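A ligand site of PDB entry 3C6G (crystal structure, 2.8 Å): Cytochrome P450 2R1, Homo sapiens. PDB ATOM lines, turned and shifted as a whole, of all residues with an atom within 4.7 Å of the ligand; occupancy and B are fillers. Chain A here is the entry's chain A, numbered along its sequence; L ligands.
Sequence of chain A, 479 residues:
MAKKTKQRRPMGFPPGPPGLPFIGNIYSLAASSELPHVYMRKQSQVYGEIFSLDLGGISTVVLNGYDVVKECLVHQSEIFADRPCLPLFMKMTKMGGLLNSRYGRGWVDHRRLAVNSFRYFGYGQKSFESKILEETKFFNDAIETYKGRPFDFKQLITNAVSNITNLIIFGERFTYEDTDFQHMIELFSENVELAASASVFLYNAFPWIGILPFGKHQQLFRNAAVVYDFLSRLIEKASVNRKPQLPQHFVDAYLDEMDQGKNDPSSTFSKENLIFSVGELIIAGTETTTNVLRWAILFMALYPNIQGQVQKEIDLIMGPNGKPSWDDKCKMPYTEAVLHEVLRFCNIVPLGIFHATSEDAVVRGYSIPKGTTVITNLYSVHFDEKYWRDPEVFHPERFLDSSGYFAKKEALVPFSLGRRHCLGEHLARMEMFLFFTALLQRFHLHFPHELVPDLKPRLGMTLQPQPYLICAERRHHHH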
ATOM      1  N   LEU A  73      35.842 -28.919  -9.259  1.00  0.00           N
ATOM      2  CA  LEU A  73      34.571 -28.243  -9.454  1.00  0.00           C
ATOM      3  C   LEU A  73      34.682 -27.038 -10.378  1.00  0.00           C
ATOM      4  O   LEU A  73      33.685 -26.655 -10.982  1.00  0.00           O
ATOM      5  CB  LEU A  73      33.941 -27.818  -8.119  1.00  0.00           C
ATOM      6  CG  LEU A  73      33.472 -28.923  -7.135  1.00  0.00           C
ATOM      7  CD1 LEU A  73      32.693 -28.311  -5.995  1.00  0.00           C
ATOM      8  CD2 LEU A  73      32.627 -30.011  -7.812  1.00  0.00           C
ATOM      9  N   ARG A  83      25.324 -35.588 -10.098  1.00  0.00           N
ATOM     10  CA  ARG A  83      24.932 -36.095  -8.785  1.00  0.00           C
ATOM     11  C   ARG A  83      24.975 -37.615  -8.826  1.00  0.00           C
ATOM     12  O   ARG A  83      24.709 -38.223  -9.861  1.00  0.00           O
ATOM     13  CB  ARG A  83      23.526 -35.674  -8.426  1.00  0.00           C
ATOM     14  CG  ARG A  83      23.315 -34.215  -8.352  1.00  0.00           C
ATOM     15  CD  ARG A  83      23.958 -33.642  -7.156  1.00  0.00           C
ATOM     16  NE  ARG A  83      23.678 -32.217  -7.060  1.00  0.00           N
ATOM     17  CZ  ARG A  83      24.407 -31.349  -6.362  1.00  0.00           C
ATOM     18  NH1 ARG A  83      25.482 -31.742  -5.686  1.00  0.00           N
ATOM     19  NH2 ARG A  83      24.053 -30.069  -6.334  1.00  0.00           N
ATOM     20  N   LEU A  98      15.764 -30.473  -9.360  1.00  0.00           N
ATOM     21  CA  LEU A  98      16.841 -29.506  -9.495  1.00  0.00           C
ATOM     22  C   LEU A  98      18.081 -29.919  -8.672  1.00  0.00           C
ATOM     23  O   LEU A  98      19.132 -30.249  -9.217  1.00  0.00           O
ATOM     24  CB  LEU A  98      16.341 -28.110  -9.075  1.00  0.00           C
ATOM     25  CG  LEU A  98      17.357 -26.951  -8.957  1.00  0.00           C
ATOM     26  CD1 LEU A  98      18.319 -26.900 -10.122  1.00  0.00           C
ATOM     27  CD2 LEU A  98      16.623 -25.617  -8.842  1.00  0.00           C
ATOM     28  N   LEU A  99      17.923 -29.918  -7.357  1.00  0.00           N
ATOM     29  CA  LEU A  99      19.056 -30.099  -6.445  1.00  0.00           C
ATOM     30  C   LEU A  99      19.797 -31.434  -6.654  1.00  0.00           C
ATOM     31  O   LEU A  99      21.027 -31.466  -6.691  1.00  0.00           O
ATOM     32  CB  LEU A  99      18.594 -29.972  -4.982  1.00  0.00           C
ATOM     33  CG  LEU A  99      19.670 -30.003  -3.896  1.00  0.00           C
ATOM     34  CD1 LEU A  99      19.266 -29.126  -2.722  1.00  0.00           C
ATOM     35  CD2 LEU A  99      19.944 -31.461  -3.440  1.00  0.00           C
ATOM     36  N   TRP A 107      18.220 -30.540 -15.656  1.00  0.00           N
ATOM     37  CA  TRP A 107      18.843 -29.622 -14.710  1.00  0.00           C
ATOM     38  C   TRP A 107      19.002 -28.236 -15.308  1.00  0.00           C
ATOM     39  O   TRP A 107      18.780 -27.254 -14.625  1.00  0.00           O
ATOM     40  CB  TRP A 107      20.203 -30.156 -14.247  1.00  0.00           C
ATOM     41  CG  TRP A 107      20.951 -29.174 -13.414  1.00  0.00           C
ATOM     42  CD1 TRP A 107      20.782 -28.939 -12.080  1.00  0.00           C
ATOM     43  CD2 TRP A 107      21.935 -28.248 -13.869  1.00  0.00           C
ATOM     44  NE1 TRP A 107      21.626 -27.937 -11.674  1.00  0.00           N
ATOM     45  CE2 TRP A 107      22.338 -27.487 -12.755  1.00  0.00           C
ATOM     46  CE3 TRP A 107      22.527 -27.991 -15.112  1.00  0.00           C
ATOM     47  CZ2 TRP A 107      23.313 -26.497 -12.846  1.00  0.00           C
ATOM     48  CZ3 TRP A 107      23.489 -27.012 -15.203  1.00  0.00           C
ATOM     49  CH2 TRP A 107      23.880 -26.281 -14.072  1.00  0.00           C
ATOM     50  N   ARG A 111      17.190 -25.304 -13.261  1.00  0.00           N
ATOM     51  CA  ARG A 111      18.120 -24.286 -12.792  1.00  0.00           C
ATOM     52  C   ARG A 111      17.764 -22.949 -13.442  1.00  0.00           C
ATOM     53  O   ARG A 111      17.480 -21.992 -12.729  1.00  0.00           O
ATOM     54  CB  ARG A 111      19.562 -24.668 -13.114  1.00  0.00           C
ATOM     55  CG  ARG A 111      20.633 -23.628 -12.734  1.00  0.00           C
ATOM     56  CD  ARG A 111      21.278 -23.933 -11.446  1.00  0.00           C
ATOM     57  NE  ARG A 111      22.323 -22.980 -11.094  1.00  0.00           N
ATOM     58  CZ  ARG A 111      23.088 -23.055  -9.992  1.00  0.00           C
ATOM     59  NH1 ARG A 111      22.939 -24.058  -9.126  1.00  0.00           N
ATOM     60  NH2 ARG A 111      24.009 -22.111  -9.768  1.00  0.00           N
ATOM     61  N   PHE A 118      13.874 -16.276  -9.106  1.00  0.00           N
ATOM     62  CA  PHE A 118      14.336 -15.626  -7.892  1.00  0.00           C
ATOM     63  C   PHE A 118      14.712 -14.175  -8.169  1.00  0.00           C
ATOM     64  O   PHE A 118      14.478 -13.300  -7.347  1.00  0.00           O
ATOM     65  CB  PHE A 118      15.495 -16.410  -7.271  1.00  0.00           C
ATOM     66  CG  PHE A 118      15.046 -17.514  -6.386  1.00  0.00           C
ATOM     67  CD1 PHE A 118      14.493 -18.654  -6.915  1.00  0.00           C
ATOM     68  CD2 PHE A 118      15.105 -17.393  -5.014  1.00  0.00           C
ATOM     69  CE1 PHE A 118      14.035 -19.689  -6.086  1.00  0.00           C
ATOM     70  CE2 PHE A 118      14.651 -18.414  -4.189  1.00  0.00           C
ATOM     71  CZ  PHE A 118      14.121 -19.554  -4.719  1.00  0.00           C
ATOM     72  N   THR A 165      11.282 -17.096   1.124  1.00  0.00           N
ATOM     73  CA  THR A 165      11.224 -17.941  -0.061  1.00  0.00           C
ATOM     74  C   THR A 165       9.760 -18.143  -0.482  1.00  0.00           C
ATOM     75  O   THR A 165       9.451 -18.112  -1.666  1.00  0.00           O
ATOM     76  CB  THR A 165      11.967 -19.277   0.142  1.00  0.00           C
ATOM     77  OG1 THR A 165      13.368 -19.026   0.238  1.00  0.00           O
ATOM     78  CG2 THR A 165      11.758 -20.186  -1.052  1.00  0.00           C
ATOM     79  N   LEU A 281      13.954 -26.223  -3.317  1.00  0.00           N
ATOM     80  CA  LEU A 281      14.115 -24.786  -3.065  1.00  0.00           C
ATOM     81  C   LEU A 281      13.722 -24.393  -1.626  1.00  0.00           C
ATOM     82  O   LEU A 281      14.449 -23.657  -0.978  1.00  0.00           O
ATOM     83  CB  LEU A 281      13.351 -23.947  -4.104  1.00  0.00           C
ATOM     84  CG  LEU A 281      13.920 -24.030  -5.541  1.00  0.00           C
ATOM     85  CD1 LEU A 281      12.871 -23.641  -6.593  1.00  0.00           C
ATOM     86  CD2 LEU A 281      15.227 -23.199  -5.732  1.00  0.00           C
ATOM     87  N   ALA A 284      16.181 -26.041   0.947  1.00  0.00           N
ATOM     88  CA  ALA A 284      17.533 -25.545   0.769  1.00  0.00           C
ATOM     89  C   ALA A 284      17.658 -24.198   1.433  1.00  0.00           C
ATOM     90  O   ALA A 284      18.671 -23.916   2.099  1.00  0.00           O
ATOM     91  CB  ALA A 284      17.860 -25.435  -0.664  1.00  0.00           C
ATOM     92  N   GLY A 285      16.626 -23.383   1.279  1.00  0.00           N
ATOM     93  CA  GLY A 285      16.594 -22.057   1.866  1.00  0.00           C
ATOM     94  C   GLY A 285      16.496 -22.121   3.375  1.00  0.00           C
ATOM     95  O   GLY A 285      17.318 -21.520   4.081  1.00  0.00           O
ATOM     96  N   THR A 288      19.506 -24.089   5.678  1.00  0.00           N
ATOM     97  CA  THR A 288      20.797 -23.465   5.698  1.00  0.00           C
ATOM     98  C   THR A 288      20.746 -22.054   6.340  1.00  0.00           C
ATOM     99  O   THR A 288      21.362 -21.799   7.387  1.00  0.00           O
ATOM    100  CB  THR A 288      21.386 -23.438   4.262  1.00  0.00           C
ATOM    101  OG1 THR A 288      20.551 -22.628   3.428  1.00  0.00           O
ATOM    102  CG2 THR A 288      21.429 -24.838   3.670  1.00  0.00           C
ATOM    103  N   THR A 289      19.991 -21.137   5.729  1.00  0.00           N
ATOM    104  CA  THR A 289      19.946 -19.772   6.231  1.00  0.00           C
ATOM    105  C   THR A 289      19.590 -19.732   7.719  1.00  0.00           C
ATOM    106  O   THR A 289      20.260 -19.058   8.503  1.00  0.00           O
ATOM    107  CB  THR A 289      18.994 -18.869   5.430  1.00  0.00           C
ATOM    108  OG1 THR A 289      19.296 -18.987   4.037  1.00  0.00           O
ATOM    109  CG2 THR A 289      19.177 -17.409   5.849  1.00  0.00           C
ATOM    110  N   VAL A 292      22.677 -20.732   9.808  1.00  0.00           N
ATOM    111  CA  VAL A 292      23.657 -19.629   9.856  1.00  0.00           C
ATOM    112  C   VAL A 292      23.302 -18.625  10.967  1.00  0.00           C
ATOM    113  O   VAL A 292      24.134 -18.298  11.818  1.00  0.00           O
ATOM    114  CB  VAL A 292      23.738 -18.877   8.549  1.00  0.00           C
ATOM    115  CG1 VAL A 292      24.470 -17.572   8.748  1.00  0.00           C
ATOM    116  CG2 VAL A 292      24.395 -19.753   7.479  1.00  0.00           C
ATOM    117  N   LEU A 343      30.115 -18.256   8.636  1.00  0.00           N
ATOM    118  CA  LEU A 343      30.082 -19.182   7.486  1.00  0.00           C
ATOM    119  C   LEU A 343      31.324 -20.025   7.443  1.00  0.00           C
ATOM    120  O   LEU A 343      31.240 -21.240   7.285  1.00  0.00           O
ATOM    121  CB  LEU A 343      29.939 -18.426   6.164  1.00  0.00           C
ATOM    122  CG  LEU A 343      28.598 -17.715   5.915  1.00  0.00           C
ATOM    123  CD1 LEU A 343      28.656 -16.935   4.621  1.00  0.00           C
ATOM    124  CD2 LEU A 343      27.425 -18.705   5.930  1.00  0.00           C
ATOM    125  N   VAL A 349      26.989 -26.172   5.700  1.00  0.00           N
ATOM    126  CA  VAL A 349      26.991 -27.328   4.788  1.00  0.00           C
ATOM    127  C   VAL A 349      28.420 -27.867   4.665  1.00  0.00           C
ATOM    128  O   VAL A 349      29.135 -27.550   3.705  1.00  0.00           O
ATOM    129  CB  VAL A 349      26.437 -27.007   3.396  1.00  0.00           C
ATOM    130  CG1 VAL A 349      26.079 -28.272   2.689  1.00  0.00           C
ATOM    131  CG2 VAL A 349      25.234 -26.094   3.504  1.00  0.00           C
ATOM    132  N   GLY A 352      29.128 -30.122   1.562  1.00  0.00           N
ATOM    133  CA  GLY A 352      28.309 -29.719   0.439  1.00  0.00           C
ATOM    134  C   GLY A 352      27.187 -30.696   0.183  1.00  0.00           C
ATOM    135  O   GLY A 352      26.672 -31.325   1.110  1.00  0.00           O
ATOM    136  N   ILE A 353      26.799 -30.795  -1.078  1.00  0.00           N
ATOM    137  CA  ILE A 353      25.873 -31.792  -1.547  1.00  0.00           C
ATOM    138  C   ILE A 353      26.723 -32.676  -2.426  1.00  0.00           C
ATOM    139  O   ILE A 353      27.481 -32.168  -3.226  1.00  0.00           O
ATOM    140  CB  ILE A 353      24.704 -31.142  -2.308  1.00  0.00           C
ATOM    141  CG1 ILE A 353      23.982 -30.149  -1.375  1.00  0.00           C
ATOM    142  CG2 ILE A 353      23.751 -32.198  -2.818  1.00  0.00           C
ATOM    143  CD1 ILE A 353      22.716 -29.505  -1.933  1.00  0.00           C
ATOM    144  N   HIS A 355      28.611 -34.770  -5.052  1.00  0.00           N
ATOM    145  CA  HIS A 355      28.689 -34.734  -6.500  1.00  0.00           C
ATOM    146  C   HIS A 355      28.952 -36.124  -7.036  1.00  0.00           C
ATOM    147  O   HIS A 355      29.144 -37.064  -6.272  1.00  0.00           O
ATOM    148  CB  HIS A 355      29.827 -33.845  -6.919  1.00  0.00           C
ATOM    149  CG  HIS A 355      29.544 -32.405  -6.757  1.00  0.00           C
ATOM    150  ND1 HIS A 355      29.458 -31.542  -7.830  1.00  0.00           N
ATOM    151  CD2 HIS A 355      29.320 -31.660  -5.651  1.00  0.00           C
ATOM    152  CE1 HIS A 355      29.192 -30.320  -7.385  1.00  0.00           C
ATOM    153  NE2 HIS A 355      29.093 -30.370  -6.076  1.00  0.00           N
ATOM    154  N   LEU A 378      34.069 -29.125   2.082  1.00  0.00           N
ATOM    155  CA  LEU A 378      34.142 -27.658   2.193  1.00  0.00           C
ATOM    156  C   LEU A 378      34.693 -27.197   3.559  1.00  0.00           C
ATOM    157  O   LEU A 378      35.381 -26.179   3.639  1.00  0.00           O
ATOM    158  CB  LEU A 378      32.771 -27.019   1.932  1.00  0.00           C
ATOM    159  CG  LEU A 378      32.075 -27.391   0.608  1.00  0.00           C
ATOM    160  CD1 LEU A 378      30.740 -26.699   0.546  1.00  0.00           C
ATOM    161  CD2 LEU A 378      32.913 -27.054  -0.584  1.00  0.00           C
ATOM    162  N   PRO A 414      31.414 -21.316   1.178  1.00  0.00           N
ATOM    163  CA  PRO A 414      30.300 -21.997   1.864  1.00  0.00           C
ATOM    164  C   PRO A 414      29.057 -22.227   0.984  1.00  0.00           C
ATOM    165  O   PRO A 414      28.151 -22.954   1.390  1.00  0.00           O
ATOM    166  CB  PRO A 414      29.969 -21.038   3.003  1.00  0.00           C
ATOM    167  CG  PRO A 414      30.369 -19.726   2.480  1.00  0.00           C
ATOM    168  CD  PRO A 414      31.602 -19.956   1.674  1.00  0.00           C
ATOM    169  N   PHE A 415      29.023 -21.596  -0.183  1.00  0.00           N
ATOM    170  CA  PHE A 415      27.992 -21.836  -1.203  1.00  0.00           C
ATOM    171  C   PHE A 415      28.562 -22.711  -2.352  1.00  0.00           C
ATOM    172  O   PHE A 415      27.984 -22.782  -3.465  1.00  0.00           O
ATOM    173  CB  PHE A 415      27.487 -20.510  -1.739  1.00  0.00           C
ATOM    174  CG  PHE A 415      26.914 -19.589  -0.668  1.00  0.00           C
ATOM    175  CD1 PHE A 415      27.693 -18.553  -0.145  1.00  0.00           C
ATOM    176  CD2 PHE A 415      25.614 -19.750  -0.210  1.00  0.00           C
ATOM    177  CE1 PHE A 415      27.177 -17.710   0.835  1.00  0.00           C
ATOM    178  CE2 PHE A 415      25.085 -18.901   0.754  1.00  0.00           C
ATOM    179  CZ  PHE A 415      25.882 -17.877   1.280  1.00  0.00           C
ATOM    180  N   SER A 416      29.700 -23.354  -2.089  1.00  0.00           N
ATOM    181  CA  SER A 416      30.360 -24.222  -3.031  1.00  0.00           C
ATOM    182  C   SER A 416      30.823 -23.469  -4.279  1.00  0.00           C
ATOM    183  O   SER A 416      30.899 -22.248  -4.255  1.00  0.00           O
ATOM    184  CB  SER A 416      29.459 -25.397  -3.401  1.00  0.00           C
ATOM    185  OG  SER A 416      30.197 -26.325  -4.162  1.00  0.00           O
ATOM    186  N   LEU A 417      31.172 -24.200  -5.340  1.00  0.00           N
ATOM    187  CA  LEU A 417      31.716 -23.639  -6.575  1.00  0.00           C
ATOM    188  C   LEU A 417      31.253 -24.421  -7.790  1.00  0.00           C
ATOM    189  O   LEU A 417      30.784 -25.564  -7.684  1.00  0.00           O
ATOM    190  CB  LEU A 417      33.258 -23.713  -6.583  1.00  0.00           C
ATOM    191  CG  LEU A 417      34.098 -23.098  -5.473  1.00  0.00           C
ATOM    192  CD1 LEU A 417      35.593 -23.449  -5.670  1.00  0.00           C
ATOM    193  CD2 LEU A 417      33.850 -21.578  -5.414  1.00  0.00           C
ATOM    194  N   ARG A 419      29.426 -25.357 -11.523  1.00  0.00           N
ATOM    195  CA  ARG A 419      28.128 -25.333 -12.191  1.00  0.00           C
ATOM    196  C   ARG A 419      26.989 -25.465 -11.215  1.00  0.00           C
ATOM    197  O   ARG A 419      25.918 -24.925 -11.444  1.00  0.00           O
ATOM    198  CB  ARG A 419      28.050 -26.451 -13.235  1.00  0.00           C
ATOM    199  CG  ARG A 419      29.044 -26.279 -14.399  1.00  0.00           C
ATOM    200  CD  ARG A 419      28.435 -25.554 -15.595  1.00  0.00           C
ATOM    201  NE  ARG A 419      29.366 -24.578 -16.163  1.00  0.00           N
ATOM    202  CZ  ARG A 419      29.042 -23.600 -17.013  1.00  0.00           C
ATOM    203  NH1 ARG A 419      27.791 -23.449 -17.452  1.00  0.00           N
ATOM    204  NH2 ARG A 419      29.980 -22.752 -17.443  1.00  0.00           N
ATOM    205  N   ARG A 420      27.233 -26.166 -10.108  1.00  0.00           N
ATOM    206  CA  ARG A 420      26.169 -26.466  -9.147  1.00  0.00           C
ATOM    207  C   ARG A 420      26.087 -25.547  -7.962  1.00  0.00           C
ATOM    208  O   ARG A 420      25.316 -25.808  -7.053  1.00  0.00           O
ATOM    209  CB  ARG A 420      26.331 -27.891  -8.648  1.00  0.00           C
ATOM    210  CG  ARG A 420      25.981 -28.907  -9.684  1.00  0.00           C
ATOM    211  CD  ARG A 420      24.493 -29.005  -9.850  1.00  0.00           C
ATOM    212  NE  ARG A 420      24.189 -30.148 -10.655  1.00  0.00           N
ATOM    213  CZ  ARG A 420      23.130 -30.942 -10.515  1.00  0.00           C
ATOM    214  NH1 ARG A 420      22.195 -30.728  -9.591  1.00  0.00           N
ATOM    215  NH2 ARG A 420      23.010 -31.962 -11.341  1.00  0.00           N
ATOM    216  N   HIS A 421      26.846 -24.455  -7.969  1.00  0.00           N
ATOM    217  CA  HIS A 421      26.975 -23.605  -6.794  1.00  0.00           C
ATOM    218  C   HIS A 421      25.628 -23.109  -6.309  1.00  0.00           C
ATOM    219  O   HIS A 421      24.680 -23.034  -7.056  1.00  0.00           O
ATOM    220  CB  HIS A 421      27.936 -22.426  -7.059  1.00  0.00           C
ATOM    221  CG  HIS A 421      27.375 -21.361  -7.938  1.00  0.00           C
ATOM    222  ND1 HIS A 421      27.330 -21.489  -9.319  1.00  0.00           N
ATOM    223  CD2 HIS A 421      26.855 -20.147  -7.650  1.00  0.00           C
ATOM    224  CE1 HIS A 421      26.787 -20.401  -9.839  1.00  0.00           C
ATOM    225  NE2 HIS A 421      26.500 -19.567  -8.857  1.00  0.00           N
ATOM    226  N   CYS A 422      25.554 -22.782  -5.031  1.00  0.00           N
ATOM    227  CA  CYS A 422      24.286 -22.349  -4.476  1.00  0.00           C
ATOM    228  C   CYS A 422      23.619 -21.338  -5.386  1.00  0.00           C
ATOM    229  O   CYS A 422      24.196 -20.362  -5.818  1.00  0.00           O
ATOM    230  CB  CYS A 422      24.411 -21.781  -3.094  1.00  0.00           C
ATOM    231  SG  CYS A 422      22.834 -21.621  -2.288  1.00  0.00           S
ATOM    232  N   LEU A 423      22.394 -21.646  -5.662  1.00  0.00           N
ATOM    233  CA  LEU A 423      21.529 -20.900  -6.528  1.00  0.00           C
ATOM    234  C   LEU A 423      20.954 -19.719  -5.785  1.00  0.00           C
ATOM    235  O   LEU A 423      20.470 -18.772  -6.403  1.00  0.00           O
ATOM    236  CB  LEU A 423      20.407 -21.853  -6.907  1.00  0.00           C
ATOM    237  CG  LEU A 423      19.235 -21.511  -7.739  1.00  0.00           C
ATOM    238  CD1 LEU A 423      18.623 -22.845  -8.158  1.00  0.00           C
ATOM    239  CD2 LEU A 423      18.254 -20.662  -6.955  1.00  0.00           C
ATOM    240  N   GLY A 424      20.990 -19.784  -4.464  1.00  0.00           N
ATOM    241  CA  GLY A 424      20.355 -18.806  -3.614  1.00  0.00           C
ATOM    242  C   GLY A 424      21.341 -17.934  -2.870  1.00  0.00           C
ATOM    243  O   GLY A 424      20.958 -17.238  -1.927  1.00  0.00           O
ATOM    244  N   LEU A 427      20.337 -14.242  -2.366  1.00  0.00           N
ATOM    245  CA  LEU A 427      19.172 -14.142  -1.465  1.00  0.00           C
ATOM    246  C   LEU A 427      19.566 -14.408  -0.007  1.00  0.00           C
ATOM    247  O   LEU A 427      19.172 -13.682   0.895  1.00  0.00           O
ATOM    248  CB  LEU A 427      18.071 -15.104  -1.897  1.00  0.00           C
ATOM    249  CG  LEU A 427      16.733 -14.905  -1.195  1.00  0.00           C
ATOM    250  CD1 LEU A 427      16.134 -13.553  -1.524  1.00  0.00           C
ATOM    251  CD2 LEU A 427      15.785 -16.025  -1.587  1.00  0.00           C
ATOM    252  N   ALA A 428      20.381 -15.430   0.209  1.00  0.00           N
ATOM    253  CA  ALA A 428      20.824 -15.808   1.555  1.00  0.00           C
ATOM    254  C   ALA A 428      21.573 -14.671   2.242  1.00  0.00           C
ATOM    255  O   ALA A 428      21.396 -14.430   3.441  1.00  0.00           O
ATOM    256  CB  ALA A 428      21.713 -17.046   1.477  1.00  0.00           C
ATOM    257  N   GLU A 431      19.130 -11.915   3.283  1.00  0.00           N
ATOM    258  CA  GLU A 431      18.408 -12.431   4.437  1.00  0.00           C
ATOM    259  C   GLU A 431      19.302 -12.352   5.664  1.00  0.00           C
ATOM    260  O   GLU A 431      18.939 -11.723   6.634  1.00  0.00           O
ATOM    261  CB  GLU A 431      17.975 -13.879   4.225  1.00  0.00           C
ATOM    262  CG  GLU A 431      16.539 -14.063   3.718  1.00  0.00           C
ATOM    263  CD  GLU A 431      16.236 -15.553   3.334  1.00  0.00           C
ATOM    264  OE1 GLU A 431      17.047 -16.167   2.586  1.00  0.00           O
ATOM    265  OE2 GLU A 431      15.187 -16.085   3.770  1.00  0.00           O
ATOM    266  N   MET A 432      20.475 -12.965   5.596  1.00  0.00           N
ATOM    267  CA  MET A 432      21.404 -12.983   6.723  1.00  0.00           C
ATOM    268  C   MET A 432      21.656 -11.590   7.291  1.00  0.00           C
ATOM    269  O   MET A 432      21.447 -11.348   8.462  1.00  0.00           O
ATOM    270  CB  MET A 432      22.742 -13.565   6.304  1.00  0.00           C
ATOM    271  CG  MET A 432      22.793 -15.041   6.312  1.00  0.00           C
ATOM    272  SD  MET A 432      24.247 -15.678   5.464  1.00  0.00           S
ATOM    273  CE  MET A 432      25.526 -14.549   6.065  1.00  0.00           C
HETATM  274  C1  LIG L   1      23.208 -25.722  -3.506  1.00  0.00           C
HETATM  275  C2  LIG L   1      24.828 -23.706   0.576  1.00  0.00           C
HETATM  276  C3  LIG L   1      20.898 -21.001   0.794  1.00  0.00           C
HETATM  277  C4  LIG L   1      19.092 -23.299  -2.967  1.00  0.00           C
HETATM  278  C5  LIG L   1      23.985 -25.413  -2.425  1.00  0.00           C
HETATM  279  C6  LIG L   1      25.265 -26.001  -2.112  1.00  0.00           C
HETATM  280  C7  LIG L   1      25.687 -25.438  -0.995  1.00  0.00           C
HETATM  281  C8  LIG L   1      24.711 -24.481  -0.570  1.00  0.00           C
HETATM  282  C9  LIG L   1      27.017 -25.781  -0.277  1.00  0.00           C
HETATM  283  C10 LIG L   1      26.045 -27.109  -2.839  1.00  0.00           C
HETATM  284  C11 LIG L   1      26.211 -26.893  -4.316  1.00  0.00           C
HETATM  285  C12 LIG L   1      26.913 -28.101  -4.875  1.00  0.00           C
HETATM  286  O1  LIG L   1      26.270 -29.090  -5.257  1.00  0.00           O
HETATM  287  O2  LIG L   1      28.145 -28.075  -4.943  1.00  0.00           O
HETATM  288  C13 LIG L   1      23.925 -22.779   0.999  1.00  0.00           C
HETATM  289  C14 LIG L   1      24.071 -21.914   2.141  1.00  0.00           C
HETATM  290  C15 LIG L   1      22.956 -21.184   2.172  1.00  0.00           C
HETATM  291  C16 LIG L   1      22.114 -21.549   1.068  1.00  0.00           C
HETATM  292  C17 LIG L   1      25.249 -21.835   3.136  1.00  0.00           C
HETATM  293  C18 LIG L   1      22.596 -20.079   3.182  1.00  0.00           C
HETATM  294  C19 LIG L   1      23.437 -19.786   4.155  1.00  0.00           C
HETATM  295  C20 LIG L   1      20.088 -21.358  -0.229  1.00  0.00           C
HETATM  296  C21 LIG L   1      18.849 -20.706  -0.588  1.00  0.00           C
HETATM  297  C22 LIG L   1      18.388 -21.379  -1.631  1.00  0.00           C
HETATM  298  C23 LIG L   1      19.293 -22.429  -1.953  1.00  0.00           C
HETATM  299  C24 LIG L   1      18.200 -19.466   0.120  1.00  0.00           C
HETATM  300  C25 LIG L   1      17.108 -21.131  -2.429  1.00  0.00           C
HETATM  301  C26 LIG L   1      16.294 -20.152  -2.118  1.00  0.00           C
HETATM  302  C27 LIG L   1      20.005 -24.150  -3.459  1.00  0.00           C
HETATM  303  C28 LIG L   1      19.771 -25.036  -4.558  1.00  0.00           C
HETATM  304  C29 LIG L   1      21.048 -25.780  -4.720  1.00  0.00           C
HETATM  305  C30 LIG L   1      21.939 -25.296  -3.706  1.00  0.00           C
HETATM  306  C31 LIG L   1      18.478 -25.190  -5.391  1.00  0.00           C
HETATM  307  C32 LIG L   1      21.326 -26.843  -5.777  1.00  0.00           C
HETATM  308  C33 LIG L   1      21.780 -26.107  -7.012  1.00  0.00           C
HETATM  309  C34 LIG L   1      22.073 -27.091  -8.097  1.00  0.00           C
HETATM  310  O3  LIG L   1      22.269 -26.664  -9.243  1.00  0.00           O
HETATM  311  O4  LIG L   1      22.098 -28.309  -7.838  1.00  0.00           O
HETATM  312  N1  LIG L   1      23.672 -24.480  -1.470  1.00  0.00           N
HETATM  313  N2  LIG L   1      22.716 -22.540   0.367  1.00  0.00           N
HETATM  314  N3  LIG L   1      20.335 -22.408  -1.077  1.00  0.00           N
HETATM  315  N4  LIG L   1      21.288 -24.320  -2.975  1.00  0.00           N
HETATM  316 FE1  LIG L   1      22.066 -23.336  -1.350  1.00  0.00          FE
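O of Leu 98 touches O4 of the ligand (3.8 Å). Leu 99 touches the ligand (O to O4, 3.5 Å). Phe 118 touches the ligand (CE2 to C26, 3.2 Å). Thr 165 touches the ligand (OG1 to C26, 3.9 Å). CD2 of Leu 281 touches C31 of the ligand (3.8 Å). CB of Ala 284 touches C4 of the ligand, at 3.4 Å. CA of Gly 285 touches C24 of the ligand, 3.5 Å away. Thr 288 touches the ligand. Thr 289 touches the ligand (OG1 to C18, 3.6 Å). Val 292 touches the ligand. CG2 of Val 349 touches C2 of the ligand, at 3.8 Å. Ile 353 touches the ligand (O to O1, 3.9 Å). Leu 378 touches the ligand (CD1 to C9, 3.9 Å). Pro 414 touches the ligand (O to C9, 3.5 Å). Phe 415 touches the ligand (CE2 to C15, 3.4 Å). Leu 423 touches the ligand. Gly 424 touches the ligand. Ala 428 touches the ligand (CB to C18, 3.6 Å). Hydrophobic or aromatic side chains within 4 Å of the ligand: Leu 98, Trp 107, Phe 118, Leu 281, Ala 284, Val 292, Val 349, Ile 353, His 355, Leu 378, Phe 415, Leu 423 and Ala 428. Of the 34 residues printed, 25 come within 4 Å of the ligand.
The backbone NH of Cys 422 is in hydrogen-bond range of the backbone carbonyl oxygen of Phe 415, at 2.9 Å. The guanidinium group of Arg 111 is in hydrogen-bond range of the backbone carbonyl oxygen of His 421 (2.9 Å). The guanidinium group (NH1) of Arg 83 lies within hydrogen-bond range of the backbone carbonyl oxygen (O) of Ile 353, at 3.2 Å. The guanidinium group (NE) of Arg 83 lies within hydrogen-bond range of the backbone carbonyl oxygen (O) of Leu 99, at 2.8 Å. The backbone carbonyl oxygen (O) of Gly 285 lies within hydrogen-bond range of the side-chain hydroxyl (OG1) of Thr 288, 3.5 Å away. The backbone carbonyl oxygen of Gly 285 is in hydrogen-bond range of the side-chain hydroxyl of Thr 289. NH1 of Arg 420 sits at hydrogen-bond distance from O of Leu 99 (3.2 Å). NH1 of Arg 420 is in hydrogen-bond range of O of Leu 98.
NH1 of Arg 420 is in salt-bridge range of O4 of the ligand (3.0 Å). An oxygen (O1) of the ligand lies within salt-bridge range of the guanidinium group (NH2) of Arg 83, 2.7 Å away. NE2 of His 355 lies within hydrogen-bond range of O2 of the ligand (2.7 Å). SG of Cys 422 binds FE1 of the ligand (2.1 Å). O3 of the ligand is in salt-bridge range of NH1 of Arg 111 (2.7 Å). An oxygen (O3) of the ligand sits at hydrogen-bond distance from the indole nitrogen of Trp 107 (2.8 Å). The side-chain hydroxyl (OG) of Ser 416 sits at hydrogen-bond distance from an oxygen (O2) of the ligand (2.8 Å).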
